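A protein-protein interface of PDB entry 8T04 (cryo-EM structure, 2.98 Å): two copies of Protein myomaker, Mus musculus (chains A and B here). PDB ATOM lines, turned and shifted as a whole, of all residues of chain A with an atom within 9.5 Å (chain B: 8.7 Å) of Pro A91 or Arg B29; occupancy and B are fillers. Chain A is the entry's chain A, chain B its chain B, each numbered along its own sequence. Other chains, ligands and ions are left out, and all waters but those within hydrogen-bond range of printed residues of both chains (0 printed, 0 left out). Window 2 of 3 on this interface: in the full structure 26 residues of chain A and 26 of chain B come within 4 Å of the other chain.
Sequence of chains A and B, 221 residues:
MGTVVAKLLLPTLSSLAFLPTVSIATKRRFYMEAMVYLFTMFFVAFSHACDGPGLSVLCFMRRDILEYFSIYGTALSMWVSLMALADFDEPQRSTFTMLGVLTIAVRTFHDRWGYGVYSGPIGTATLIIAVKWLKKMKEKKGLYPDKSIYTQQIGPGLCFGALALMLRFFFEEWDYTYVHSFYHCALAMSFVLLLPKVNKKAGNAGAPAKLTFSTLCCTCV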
ATOM      1  N   PHE A  88      15.823   7.380 -10.296  1.00  0.00           N
ATOM      2  CA  PHE A  88      15.863   6.773  -8.938  1.00  0.00           C
ATOM      3  C   PHE A  88      14.973   5.525  -8.906  1.00  0.00           C
ATOM      4  O   PHE A  88      14.031   5.437  -9.719  1.00  0.00           O
ATOM      5  CB  PHE A  88      15.425   7.777  -7.866  1.00  0.00           C
ATOM      6  CG  PHE A  88      16.437   8.852  -7.563  1.00  0.00           C
ATOM      7  CD1 PHE A  88      17.506   8.597  -6.716  1.00  0.00           C
ATOM      8  CD2 PHE A  88      16.322  10.118  -8.121  1.00  0.00           C
ATOM      9  CE1 PHE A  88      18.438   9.584  -6.435  1.00  0.00           C
ATOM     10  CE2 PHE A  88      17.256  11.104  -7.838  1.00  0.00           C
ATOM     11  CZ  PHE A  88      18.312  10.835  -6.996  1.00  0.00           C
ATOM     12  N   ASP A  89      15.277   4.595  -7.992  1.00  0.00           N
ATOM     13  CA  ASP A  89      14.454   3.393  -7.669  1.00  0.00           C
ATOM     14  C   ASP A  89      13.872   3.564  -6.254  1.00  0.00           C
ATOM     15  O   ASP A  89      14.193   4.581  -5.605  1.00  0.00           O
ATOM     16  CB  ASP A  89      15.247   2.094  -7.856  1.00  0.00           C
ATOM     17  CG  ASP A  89      16.578   2.030  -7.122  1.00  0.00           C
ATOM     18  OD1 ASP A  89      17.083   0.906  -6.929  1.00  0.00           O
ATOM     19  OD2 ASP A  89      17.103   3.101  -6.756  1.00  0.00           O
ATOM     20  N   GLU A  90      13.059   2.601  -5.790  1.00  0.00           N
ATOM     21  CA  GLU A  90      12.008   2.813  -4.753  1.00  0.00           C
ATOM     22  C   GLU A  90      12.727   2.452  -3.451  1.00  0.00           C
ATOM     23  O   GLU A  90      13.489   1.478  -3.392  1.00  0.00           O
ATOM     24  CB  GLU A  90      10.742   1.995  -5.042  1.00  0.00           C
ATOM     25  CG  GLU A  90       9.863   2.523  -6.159  1.00  0.00           C
ATOM     26  CD  GLU A  90       8.942   3.675  -5.795  1.00  0.00           C
ATOM     27  OE1 GLU A  90       8.529   4.404  -6.719  1.00  0.00           O
ATOM     28  OE2 GLU A  90       8.625   3.840  -4.598  1.00  0.00           O
ATOM     29  N   PRO A  91      12.559   3.277  -2.393  1.00  0.00           N
ATOM     30  CA  PRO A  91      11.477   4.188  -2.025  1.00  0.00           C
ATOM     31  C   PRO A  91      11.815   5.666  -2.314  1.00  0.00           C
ATOM     32  O   PRO A  91      11.000   6.505  -1.972  1.00  0.00           O
ATOM     33  CB  PRO A  91      11.328   3.924  -0.525  1.00  0.00           C
ATOM     34  CG  PRO A  91      12.753   3.695  -0.066  1.00  0.00           C
ATOM     35  CD  PRO A  91      13.515   3.159  -1.273  1.00  0.00           C
ATOM     36  N   GLN A  92      12.966   5.955  -2.941  1.00  0.00           N
ATOM     37  CA  GLN A  92      13.474   7.338  -3.186  1.00  0.00           C
ATOM     38  C   GLN A  92      12.691   7.999  -4.330  1.00  0.00           C
ATOM     39  O   GLN A  92      12.404   9.209  -4.207  1.00  0.00           O
ATOM     40  CB  GLN A  92      14.976   7.333  -3.491  1.00  0.00           C
ATOM     41  CG  GLN A  92      15.841   7.026  -2.274  1.00  0.00           C
ATOM     42  CD  GLN A  92      17.241   6.589  -2.632  1.00  0.00           C
ATOM     43  OE1 GLN A  92      18.222   7.245  -2.284  1.00  0.00           O
ATOM     44  NE2 GLN A  92      17.348   5.469  -3.330  1.00  0.00           N
ATOM     45  N   ARG A  93      12.366   7.247  -5.390  1.00  0.00           N
ATOM     46  CA  ARG A  93      11.672   7.748  -6.613  1.00  0.00           C
ATOM     47  C   ARG A  93      10.396   8.504  -6.223  1.00  0.00           C
ATOM     48  O   ARG A  93      10.240   9.662  -6.662  1.00  0.00           O
ATOM     49  CB  ARG A  93      11.321   6.599  -7.564  1.00  0.00           C
ATOM     50  CG  ARG A  93      11.123   7.029  -9.011  1.00  0.00           C
ATOM     51  CD  ARG A  93      10.907   5.838  -9.928  1.00  0.00           C
ATOM     52  NE  ARG A  93      11.746   5.909 -11.121  1.00  0.00           N
ATOM     53  CZ  ARG A  93      11.414   6.460 -12.291  1.00  0.00           C
ATOM     54  NH1 ARG A  93      10.227   7.019 -12.481  1.00  0.00           N
ATOM     55  NH2 ARG A  93      12.289   6.446 -13.285  1.00  0.00           N
ATOM     56  N   SER A  94       9.584   7.782  -5.421  1.00  0.00           N
ATOM     57  CA  SER A  94       8.309   8.330  -4.887  1.00  0.00           C
ATOM     58  C   SER A  94       8.586   9.495  -3.928  1.00  0.00           C
ATOM     59  O   SER A  94       7.770  10.438  -3.917  1.00  0.00           O
ATOM     60  CB  SER A  94       7.473   7.268  -4.223  1.00  0.00           C
ATOM     61  OG  SER A  94       6.869   6.423  -5.190  1.00  0.00           O
ATOM     62  N   THR A  95       9.680   9.437  -3.156  1.00  0.00           N
ATOM     63  CA  THR A  95      10.051  10.494  -2.174  1.00  0.00           C
ATOM     64  C   THR A  95      10.505  11.758  -2.914  1.00  0.00           C
ATOM     65  O   THR A  95      10.063  12.852  -2.505  1.00  0.00           O
ATOM     66  CB  THR A  95      11.111  10.023  -1.169  1.00  0.00           C
ATOM     67  OG1 THR A  95      10.675   8.788  -0.598  1.00  0.00           O
ATOM     68  CG2 THR A  95      11.345  11.028  -0.062  1.00  0.00           C
ATOM     69  N   PHE A  96      11.352  11.624  -3.941  1.00  0.00           N
ATOM     70  CA  PHE A  96      11.865  12.772  -4.735  1.00  0.00           C
ATOM     71  C   PHE A  96      10.730  13.359  -5.583  1.00  0.00           C
ATOM     72  O   PHE A  96      10.672  14.597  -5.655  1.00  0.00           O
ATOM     73  CB  PHE A  96      13.105  12.397  -5.556  1.00  0.00           C
ATOM     74  CG  PHE A  96      14.387  12.416  -4.760  1.00  0.00           C
ATOM     75  CD1 PHE A  96      14.830  13.587  -4.160  1.00  0.00           C
ATOM     76  CD2 PHE A  96      15.150  11.267  -4.601  1.00  0.00           C
ATOM     77  CE1 PHE A  96      16.003  13.607  -3.417  1.00  0.00           C
ATOM     78  CE2 PHE A  96      16.323  11.289  -3.860  1.00  0.00           C
ATOM     79  CZ  PHE A  96      16.748  12.459  -3.270  1.00  0.00           C
ATOM     80  N   THR A  97       9.848  12.529  -6.157  1.00  0.00           N
ATOM     81  CA  THR A  97       8.634  13.000  -6.885  1.00  0.00           C
ATOM     82  C   THR A  97       7.786  13.877  -5.956  1.00  0.00           C
ATOM     83  O   THR A  97       7.401  14.979  -6.390  1.00  0.00           O
ATOM     84  CB  THR A  97       7.787  11.853  -7.455  1.00  0.00           C
ATOM     85  OG1 THR A  97       8.627  11.048  -8.284  1.00  0.00           O
ATOM     86  CG2 THR A  97       6.601  12.353  -8.256  1.00  0.00           C
ATOM     87  N   MET A  98       7.517  13.408  -4.733  1.00  0.00           N
ATOM     88  CA  MET A  98       6.646  14.101  -3.745  1.00  0.00           C
ATOM     89  C   MET A  98       7.332  15.374  -3.234  1.00  0.00           C
ATOM     90  O   MET A  98       6.613  16.366  -3.008  1.00  0.00           O
ATOM     91  CB  MET A  98       6.308  13.183  -2.565  1.00  0.00           C
ATOM     92  CG  MET A  98       5.174  13.694  -1.685  1.00  0.00           C
ATOM     93  SD  MET A  98       3.537  13.154  -2.251  1.00  0.00           S
ATOM     94  CE  MET A  98       3.166  14.383  -3.501  1.00  0.00           C
ATOM     95  N   LEU A  99       8.659  15.353  -3.066  1.00  0.00           N
ATOM     96  CA  LEU A  99       9.463  16.519  -2.605  1.00  0.00           C
ATOM     97  C   LEU A  99       9.257  17.703  -3.560  1.00  0.00           C
ATOM     98  O   LEU A  99       9.035  18.820  -3.058  1.00  0.00           O
ATOM     99  CB  LEU A  99      10.938  16.111  -2.514  1.00  0.00           C
ATOM    100  CG  LEU A  99      11.915  17.222  -2.137  1.00  0.00           C
ATOM    101  CD1 LEU A  99      11.680  17.730  -0.722  1.00  0.00           C
ATOM    102  CD2 LEU A  99      13.352  16.749  -2.306  1.00  0.00           C
ATOM    103  N   VAL B  22       3.580   9.964  11.264  1.00  0.00           N
ATOM    104  CA  VAL B  22       4.839  10.243  10.505  1.00  0.00           C
ATOM    105  C   VAL B  22       5.892   9.192  10.885  1.00  0.00           C
ATOM    106  O   VAL B  22       6.491   8.612   9.956  1.00  0.00           O
ATOM    107  CB  VAL B  22       5.352  11.679  10.739  1.00  0.00           C
ATOM    108  CG1 VAL B  22       6.759  11.894  10.195  1.00  0.00           C
ATOM    109  CG2 VAL B  22       4.410  12.713  10.141  1.00  0.00           C
ATOM    110  N   SER B  23       6.111   8.961  12.186  1.00  0.00           N
ATOM    111  CA  SER B  23       7.162   8.044  12.711  1.00  0.00           C
ATOM    112  C   SER B  23       6.839   6.592  12.337  1.00  0.00           C
ATOM    113  O   SER B  23       7.778   5.879  11.932  1.00  0.00           O
ATOM    114  CB  SER B  23       7.360   8.203  14.199  1.00  0.00           C
ATOM    115  OG  SER B  23       6.172   7.878  14.907  1.00  0.00           O
ATOM    116  N   ILE B  24       5.572   6.172  12.456  1.00  0.00           N
ATOM    117  CA  ILE B  24       5.112   4.791  12.108  1.00  0.00           C
ATOM    118  C   ILE B  24       5.237   4.586  10.591  1.00  0.00           C
ATOM    119  O   ILE B  24       5.706   3.504  10.195  1.00  0.00           O
ATOM    120  CB  ILE B  24       3.691   4.505  12.643  1.00  0.00           C
ATOM    121  CG1 ILE B  24       3.701   4.395  14.172  1.00  0.00           C
ATOM    122  CG2 ILE B  24       3.092   3.255  12.003  1.00  0.00           C
ATOM    123  CD1 ILE B  24       2.335   4.442  14.821  1.00  0.00           C
ATOM    124  N   ALA B  25       4.844   5.572   9.775  1.00  0.00           N
ATOM    125  CA  ALA B  25       4.938   5.517   8.295  1.00  0.00           C
ATOM    126  C   ALA B  25       6.409   5.425   7.867  1.00  0.00           C
ATOM    127  O   ALA B  25       6.706   4.611   6.970  1.00  0.00           O
ATOM    128  CB  ALA B  25       4.250   6.705   7.665  1.00  0.00           C
ATOM    129  N   THR B  26       7.293   6.217   8.488  1.00  0.00           N
ATOM    130  CA  THR B  26       8.769   6.187   8.271  1.00  0.00           C
ATOM    131  C   THR B  26       9.308   4.789   8.606  1.00  0.00           C
ATOM    132  O   THR B  26      10.071   4.236   7.788  1.00  0.00           O
ATOM    133  CB  THR B  26       9.485   7.262   9.101  1.00  0.00           C
ATOM    134  OG1 THR B  26       8.903   8.527   8.787  1.00  0.00           O
ATOM    135  CG2 THR B  26      10.977   7.319   8.848  1.00  0.00           C
ATOM    136  N   LYS B  27       8.912   4.260   9.769  1.00  0.00           N
ATOM    137  CA  LYS B  27       9.360   2.963  10.351  1.00  0.00           C
ATOM    138  C   LYS B  27       8.959   1.784   9.448  1.00  0.00           C
ATOM    139  O   LYS B  27       9.719   0.793   9.430  1.00  0.00           O
ATOM    140  CB  LYS B  27       8.772   2.841  11.760  1.00  0.00           C
ATOM    141  CG  LYS B  27       9.184   1.626  12.579  1.00  0.00           C
ATOM    142  CD  LYS B  27       8.419   1.514  13.888  1.00  0.00           C
ATOM    143  CE  LYS B  27       8.633   2.689  14.823  1.00  0.00           C
ATOM    144  NZ  LYS B  27       7.887   2.528  16.093  1.00  0.00           N
ATOM    145  N   ARG B  28       7.830   1.879   8.733  1.00  0.00           N
ATOM    146  CA  ARG B  28       7.312   0.822   7.814  1.00  0.00           C
ATOM    147  C   ARG B  28       7.802   1.046   6.375  1.00  0.00           C
ATOM    148  O   ARG B  28       7.268   0.367   5.470  1.00  0.00           O
ATOM    149  CB  ARG B  28       5.780   0.806   7.824  1.00  0.00           C
ATOM    150  CG  ARG B  28       5.170   0.460   9.171  1.00  0.00           C
ATOM    151  CD  ARG B  28       3.662   0.501   9.102  1.00  0.00           C
ATOM    152  NE  ARG B  28       3.037   0.313  10.404  1.00  0.00           N
ATOM    153  CZ  ARG B  28       1.725   0.255  10.625  1.00  0.00           C
ATOM    154  NH1 ARG B  28       0.863   0.371   9.625  1.00  0.00           N
ATOM    155  NH2 ARG B  28       1.276   0.080  11.858  1.00  0.00           N
ATOM    156  N   ARG B  29       8.766   1.952   6.165  1.00  0.00           N
ATOM    157  CA  ARG B  29       9.377   2.272   4.845  1.00  0.00           C
ATOM    158  C   ARG B  29       8.353   2.949   3.913  1.00  0.00           C
ATOM    159  O   ARG B  29       8.569   2.896   2.684  1.00  0.00           O
ATOM    160  CB  ARG B  29       9.967   1.005   4.206  1.00  0.00           C
ATOM    161  CG  ARG B  29      10.987   0.255   5.060  1.00  0.00           C
ATOM    162  CD  ARG B  29      12.409   0.794   4.950  1.00  0.00           C
ATOM    163  NE  ARG B  29      12.944   0.624   3.601  1.00  0.00           N
ATOM    164  CZ  ARG B  29      14.146   1.019   3.172  1.00  0.00           C
ATOM    165  NH1 ARG B  29      14.488   0.797   1.912  1.00  0.00           N
ATOM    166  NH2 ARG B  29      15.001   1.627   3.982  1.00  0.00           N
ATOM    167  N   PHE B  30       7.299   3.583   4.455  1.00  0.00           N
ATOM    168  CA  PHE B  30       6.321   4.419   3.700  1.00  0.00           C
ATOM    169  C   PHE B  30       6.773   5.883   3.786  1.00  0.00           C
ATOM    170  O   PHE B  30       6.126   6.689   4.489  1.00  0.00           O
ATOM    171  CB  PHE B  30       4.892   4.231   4.225  1.00  0.00           C
ATOM    172  CG  PHE B  30       4.233   2.930   3.842  1.00  0.00           C
ATOM    173  CD1 PHE B  30       3.787   2.716   2.546  1.00  0.00           C
ATOM    174  CD2 PHE B  30       4.034   1.928   4.782  1.00  0.00           C
ATOM    175  CE1 PHE B  30       3.171   1.523   2.194  1.00  0.00           C
ATOM    176  CE2 PHE B  30       3.419   0.736   4.429  1.00  0.00           C
ATOM    177  CZ  PHE B  30       2.989   0.535   3.136  1.00  0.00           C
ATOM    178  N   TYR B  31       7.866   6.208   3.089  1.00  0.00           N
ATOM    179  CA  TYR B  31       8.587   7.507   3.183  1.00  0.00           C
ATOM    180  C   TYR B  31       7.784   8.622   2.500  1.00  0.00           C
ATOM    181  O   TYR B  31       7.702   9.720   3.085  1.00  0.00           O
ATOM    182  CB  TYR B  31       9.996   7.392   2.598  1.00  0.00           C
ATOM    183  CG  TYR B  31      10.941   6.559   3.426  1.00  0.00           C
ATOM    184  CD1 TYR B  31      11.503   7.062   4.589  1.00  0.00           C
ATOM    185  CD2 TYR B  31      11.271   5.264   3.055  1.00  0.00           C
ATOM    186  CE1 TYR B  31      12.370   6.304   5.361  1.00  0.00           C
ATOM    187  CE2 TYR B  31      12.139   4.493   3.812  1.00  0.00           C
ATOM    188  CZ  TYR B  31      12.689   5.013   4.971  1.00  0.00           C
ATOM    189  OH  TYR B  31      13.542   4.256   5.722  1.00  0.00           O
ATOM    190  N   MET B  32       7.227   8.361   1.312  1.00  0.00           N
ATOM    191  CA  MET B  32       6.429   9.351   0.532  1.00  0.00           C
ATOM    192  C   MET B  32       5.154   9.715   1.305  1.00  0.00           C
ATOM    193  O   MET B  32       4.754  10.892   1.243  1.00  0.00           O
ATOM    194  CB  MET B  32       6.058   8.809  -0.853  1.00  0.00           C
ATOM    195  CG  MET B  32       5.231   9.778  -1.688  1.00  0.00           C
ATOM    196  SD  MET B  32       3.443   9.495  -1.567  1.00  0.00           S
ATOM    197  CE  MET B  32       3.279   8.004  -2.546  1.00  0.00           C
ATOM    198  N   GLU B  33       4.541   8.746   1.994  1.00  0.00           N
ATOM    199  CA  GLU B  33       3.331   8.960   2.834  1.00  0.00           C
ATOM    200  C   GLU B  33       3.723   9.772   4.074  1.00  0.00           C
ATOM    201  O   GLU B  33       2.923  10.636   4.480  1.00  0.00           O
ATOM    202  CB  GLU B  33       2.678   7.630   3.225  1.00  0.00           C
ATOM    203  CG  GLU B  33       2.015   6.901   2.064  1.00  0.00           C
ATOM    204  CD  GLU B  33       2.937   6.171   1.099  1.00  0.00           C
ATOM    205  OE1 GLU B  33       4.142   6.043   1.402  1.00  0.00           O
ATOM    206  OE2 GLU B  33       2.446   5.733   0.038  1.00  0.00           O
ATOM    207  N   ALA B  34       4.909   9.513   4.640  1.00  0.00           N
ATOM    208  CA  ALA B  34       5.463  10.219   5.823  1.00  0.00           C
ATOM    209  C   ALA B  34       5.742  11.693   5.495  1.00  0.00           C
ATOM    210  O   ALA B  34       5.590  12.524   6.414  1.00  0.00           O
ATOM    211  CB  ALA B  34       6.702   9.518   6.327  1.00  0.00           C
ATOM    212  N   MET B  35       6.138  12.012   4.253  1.00  0.00           N
ATOM    213  CA  MET B  35       6.297  13.412   3.764  1.00  0.00           C
ATOM    214  C   MET B  35       4.943  14.127   3.828  1.00  0.00           C
ATOM    215  O   MET B  35       4.891  15.242   4.386  1.00  0.00           O
ATOM    216  CB  MET B  35       6.795  13.483   2.316  1.00  0.00           C
ATOM    217  CG  MET B  35       8.214  13.004   2.114  1.00  0.00           C
ATOM    218  SD  MET B  35       8.919  13.644   0.573  1.00  0.00           S
ATOM    219  CE  MET B  35       9.313  15.324   1.058  1.00  0.00           C
ATOM    220  N   ARG B  93       1.041   2.764  -9.739  1.00  0.00           N
ATOM    221  CA  ARG B  93       1.274   3.347  -8.384  1.00  0.00           C
ATOM    222  C   ARG B  93       1.552   4.851  -8.498  1.00  0.00           C
ATOM    223  O   ARG B  93       0.862   5.631  -7.811  1.00  0.00           O
ATOM    224  CB  ARG B  93       2.447   2.658  -7.676  1.00  0.00           C
ATOM    225  CG  ARG B  93       2.418   2.788  -6.160  1.00  0.00           C
ATOM    226  CD  ARG B  93       3.524   1.980  -5.505  1.00  0.00           C
ATOM    227  NE  ARG B  93       3.025   1.169  -4.397  1.00  0.00           N
ATOM    228  CZ  ARG B  93       2.972   1.532  -3.113  1.00  0.00           C
ATOM    229  NH1 ARG B  93       3.391   2.723  -2.711  1.00  0.00           N
ATOM    230  NH2 ARG B  93       2.489   0.681  -2.219  1.00  0.00           N
ATOM    231  N   LEU B 195      -2.810   2.305   6.728  1.00  0.00           N
ATOM    232  CA  LEU B 195      -1.450   2.094   6.159  1.00  0.00           C
ATOM    233  C   LEU B 195      -1.023   0.652   6.434  1.00  0.00           C
ATOM    234  O   LEU B 195      -1.101   0.210   7.579  1.00  0.00           O
ATOM    235  CB  LEU B 195      -0.486   3.104   6.794  1.00  0.00           C
ATOM    236  CG  LEU B 195       0.876   3.257   6.120  1.00  0.00           C
ATOM    237  CD1 LEU B 195       0.742   3.939   4.765  1.00  0.00           C
ATOM    238  CD2 LEU B 195       1.825   4.043   7.012  1.00  0.00           C
ATOM    239  N   PRO B 196      -0.595  -0.139   5.414  1.00  0.00           N
ATOM    240  CA  PRO B 196      -0.162  -1.525   5.632  1.00  0.00           C
ATOM    241  C   PRO B 196       1.033  -1.695   6.584  1.00  0.00           C
ATOM    242  O   PRO B 196       1.622  -0.705   6.971  1.00  0.00           O
ATOM    243  CB  PRO B 196       0.246  -2.019   4.234  1.00  0.00           C
ATOM    244  CG  PRO B 196      -0.512  -1.120   3.288  1.00  0.00           C
ATOM    245  CD  PRO B 196      -0.555   0.223   3.986  1.00  0.00           C
ATOM    246  N   LYS B 197       1.368  -2.947   6.911  1.00  0.00           N
ATOM    247  CA  LYS B 197       2.397  -3.310   7.926  1.00  0.00           C
ATOM    248  C   LYS B 197       3.809  -3.067   7.372  1.00  0.00           C
ATOM    249  O   LYS B 197       4.676  -2.653   8.167  1.00  0.00           O
ATOM    250  CB  LYS B 197       2.205  -4.761   8.385  1.00  0.00           C
ATOM    251  CG  LYS B 197       0.983  -4.994   9.264  1.00  0.00           C
ATOM    252  CD  LYS B 197       1.139  -4.473  10.680  1.00  0.00           C
ATOM    253  CE  LYS B 197      -0.081  -4.734  11.539  1.00  0.00           C
ATOM    254  NZ  LYS B 197       0.162  -4.393  12.961  1.00  0.00           N
ATOM    255  N   VAL B 198       4.036  -3.325   6.076  1.00  0.00           N
ATOM    256  CA  VAL B 198       5.341  -3.109   5.378  1.00  0.00           C
ATOM    257  C   VAL B 198       5.069  -2.496   3.998  1.00  0.00           C
ATOM    258  O   VAL B 198       4.096  -2.928   3.345  1.00  0.00           O
ATOM    259  CB  VAL B 198       6.141  -4.424   5.253  1.00  0.00           C
ATOM    260  CG1 VAL B 198       7.450  -4.238   4.494  1.00  0.00           C
ATOM    261  CG2 VAL B 198       6.414  -5.061   6.607  1.00  0.00           C
ATOM    262  N   ASN B 199       5.906  -1.541   3.573  1.00  0.00           N
ATOM    263  CA  ASN B 199       5.970  -1.055   2.169  1.00  0.00           C
ATOM    264  C   ASN B 199       6.714  -2.122   1.355  1.00  0.00           C
ATOM    265  O   ASN B 199       7.958  -2.059   1.287  1.00  0.00           O
ATOM    266  CB  ASN B 199       6.611   0.333   2.061  1.00  0.00           C
ATOM    267  CG  ASN B 199       6.521   0.938   0.673  1.00  0.00           C
ATOM    268  OD1 ASN B 199       5.860   0.399  -0.214  1.00  0.00           O
ATOM    269  ND2 ASN B 199       7.177   2.071   0.471  1.00  0.00           N
ATOM    270  N   LYS B 200       5.969  -3.071   0.778  1.00  0.00           N
ATOM    271  CA  LYS B 200       6.514  -4.269   0.075  1.00  0.00           C
ATOM    272  C   LYS B 200       7.230  -3.870  -1.225  1.00  0.00           C
ATOM    273  O   LYS B 200       7.990  -4.713  -1.742  1.00  0.00           O
ATOM    274  CB  LYS B 200       5.402  -5.290  -0.185  1.00  0.00           C
ATOM    275  CG  LYS B 200       4.998  -6.072   1.057  1.00  0.00           C
ATOM    276  CD  LYS B 200       3.810  -6.983   0.882  1.00  0.00           C
ATOM    277  CE  LYS B 200       3.524  -7.769   2.144  1.00  0.00           C
ATOM    278  NZ  LYS B 200       2.227  -8.482   2.075  1.00  0.00           N
ATOM    279  N   LYS B 201       7.012  -2.648  -1.726  1.00  0.00           N
ATOM    280  CA  LYS B 201       7.693  -2.104  -2.933  1.00  0.00           C
ATOM    281  C   LYS B 201       9.052  -1.484  -2.563  1.00  0.00           C
ATOM    282  O   LYS B 201       9.802  -1.161  -3.507  1.00  0.00           O
ATOM    283  CB  LYS B 201       6.798  -1.075  -3.635  1.00  0.00           C
ATOM    284  CG  LYS B 201       5.367  -1.521  -3.922  1.00  0.00           C
ATOM    285  CD  LYS B 201       5.241  -2.855  -4.635  1.00  0.00           C
ATOM    286  CE  LYS B 201       3.800  -3.279  -4.827  1.00  0.00           C
ATOM    287  NZ  LYS B 201       3.690  -4.651  -5.376  1.00  0.00           N
ATOM    288  N   ALA B 202       9.367  -1.321  -1.267  1.00  0.00           N
ATOM    289  CA  ALA B 202      10.600  -0.644  -0.788  1.00  0.00           C
ATOM    290  C   ALA B 202      11.115  -1.202   0.553  1.00  0.00           C
ATOM    291  O   ALA B 202      11.896  -0.483   1.215  1.00  0.00           O
ATOM    292  CB  ALA B 202      10.317   0.835  -0.683  1.00  0.00           C
ATOM    293  N   GLY B 203      10.742  -2.429   0.939  1.00  0.00           N
ATOM    294  CA  GLY B 203      11.140  -3.033   2.228  1.00  0.00           C
ATOM    295  C   GLY B 203      10.664  -4.470   2.371  1.00  0.00           C
ATOM    296  O   GLY B 203       9.971  -5.016   1.512  1.00  0.00           O
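Printed residues of chain B within 4 Å of Glu A90: Lys B201. Pro A91 touches just these residues of chain B: Arg B29, Tyr B31 and Ala B202. Of the printed residues of chain B, Thr A95 touches Tyr B31, Met B32 and Met B35. Arg B29 touches one residue of chain A. No residue of chain A comes within 4 Å of Asn B199. The nearest residue of chain B that does not touch Pro A91 is Asn B199 (4.7 Å).
The backbone carbonyl oxygen (O) of Thr A95 sits close to the side-chain sulfur (SD) of Met B35 (3.4 Å). SD of Met A98 lies close to SD of Met B32, 3.7 Å away.
CB of Glu A90 touches O of Lys B201, at 3.6 Å. Arg B29 touches Pro A91 (NH1 to CG, 3.9 Å). Tyr B31 touches Pro A91. Pro A91 touches Ala B202. Ser A94 touches Met B32. Tyr B31 touches Thr A95 (CB to OG1, 3.6 Å). N of Met B32 touches OG1 of Thr A95 (3.96 Å). Met B35 touches Leu A99 (CE to CD1, 3.8 Å).
Printed residues of chain B that touch a printed residue of chain A: Arg B29, Tyr B31, Met B32, Met B35, Lys B201 and Ala B202. Hydrophobic or aromatic side chains of chain B that line the printed part of chain A: Tyr B31, Met B32, Met B35 and Ala B202. Of the 12 printed residues of chain A, 6 touch a printed residue of chain B. Printed residues of chain A that touch a printed residue of chain B: Glu A90, Pro A91, Ser A94, Thr A95, Met A98 and Leu A99. Among the printed residues, no Asp or Glu carboxylate lies within 4 Å of a Lys or Arg side-chain nitrogen of the other chain.
The side-chain carboxylate (OE1) of Glu A90 sits at hydrogen-bond distance from the side-chain hydroxyl (OG) of Ser A94 (3.0 Å). OH of Tyr B31 sits at hydrogen-bond distance from NH2 of Arg B29 (3.5 Å). The side-chain hydroxyl (OG1) of Thr A95 is in hydrogen-bond range of the backbone carbonyl oxygen (O) of Pro A91 (2.7 Å). ND2 of Asn B199 is in hydrogen-bond range of O of Arg B29 (2.7 Å). O of Ala B202 sits at hydrogen-bond distance from NE of Arg B29.
Position printed for both chains: 93. Of the 10 pairs that touch across the chains among the printed residues, none has its exchanged pair printed and touching as well.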
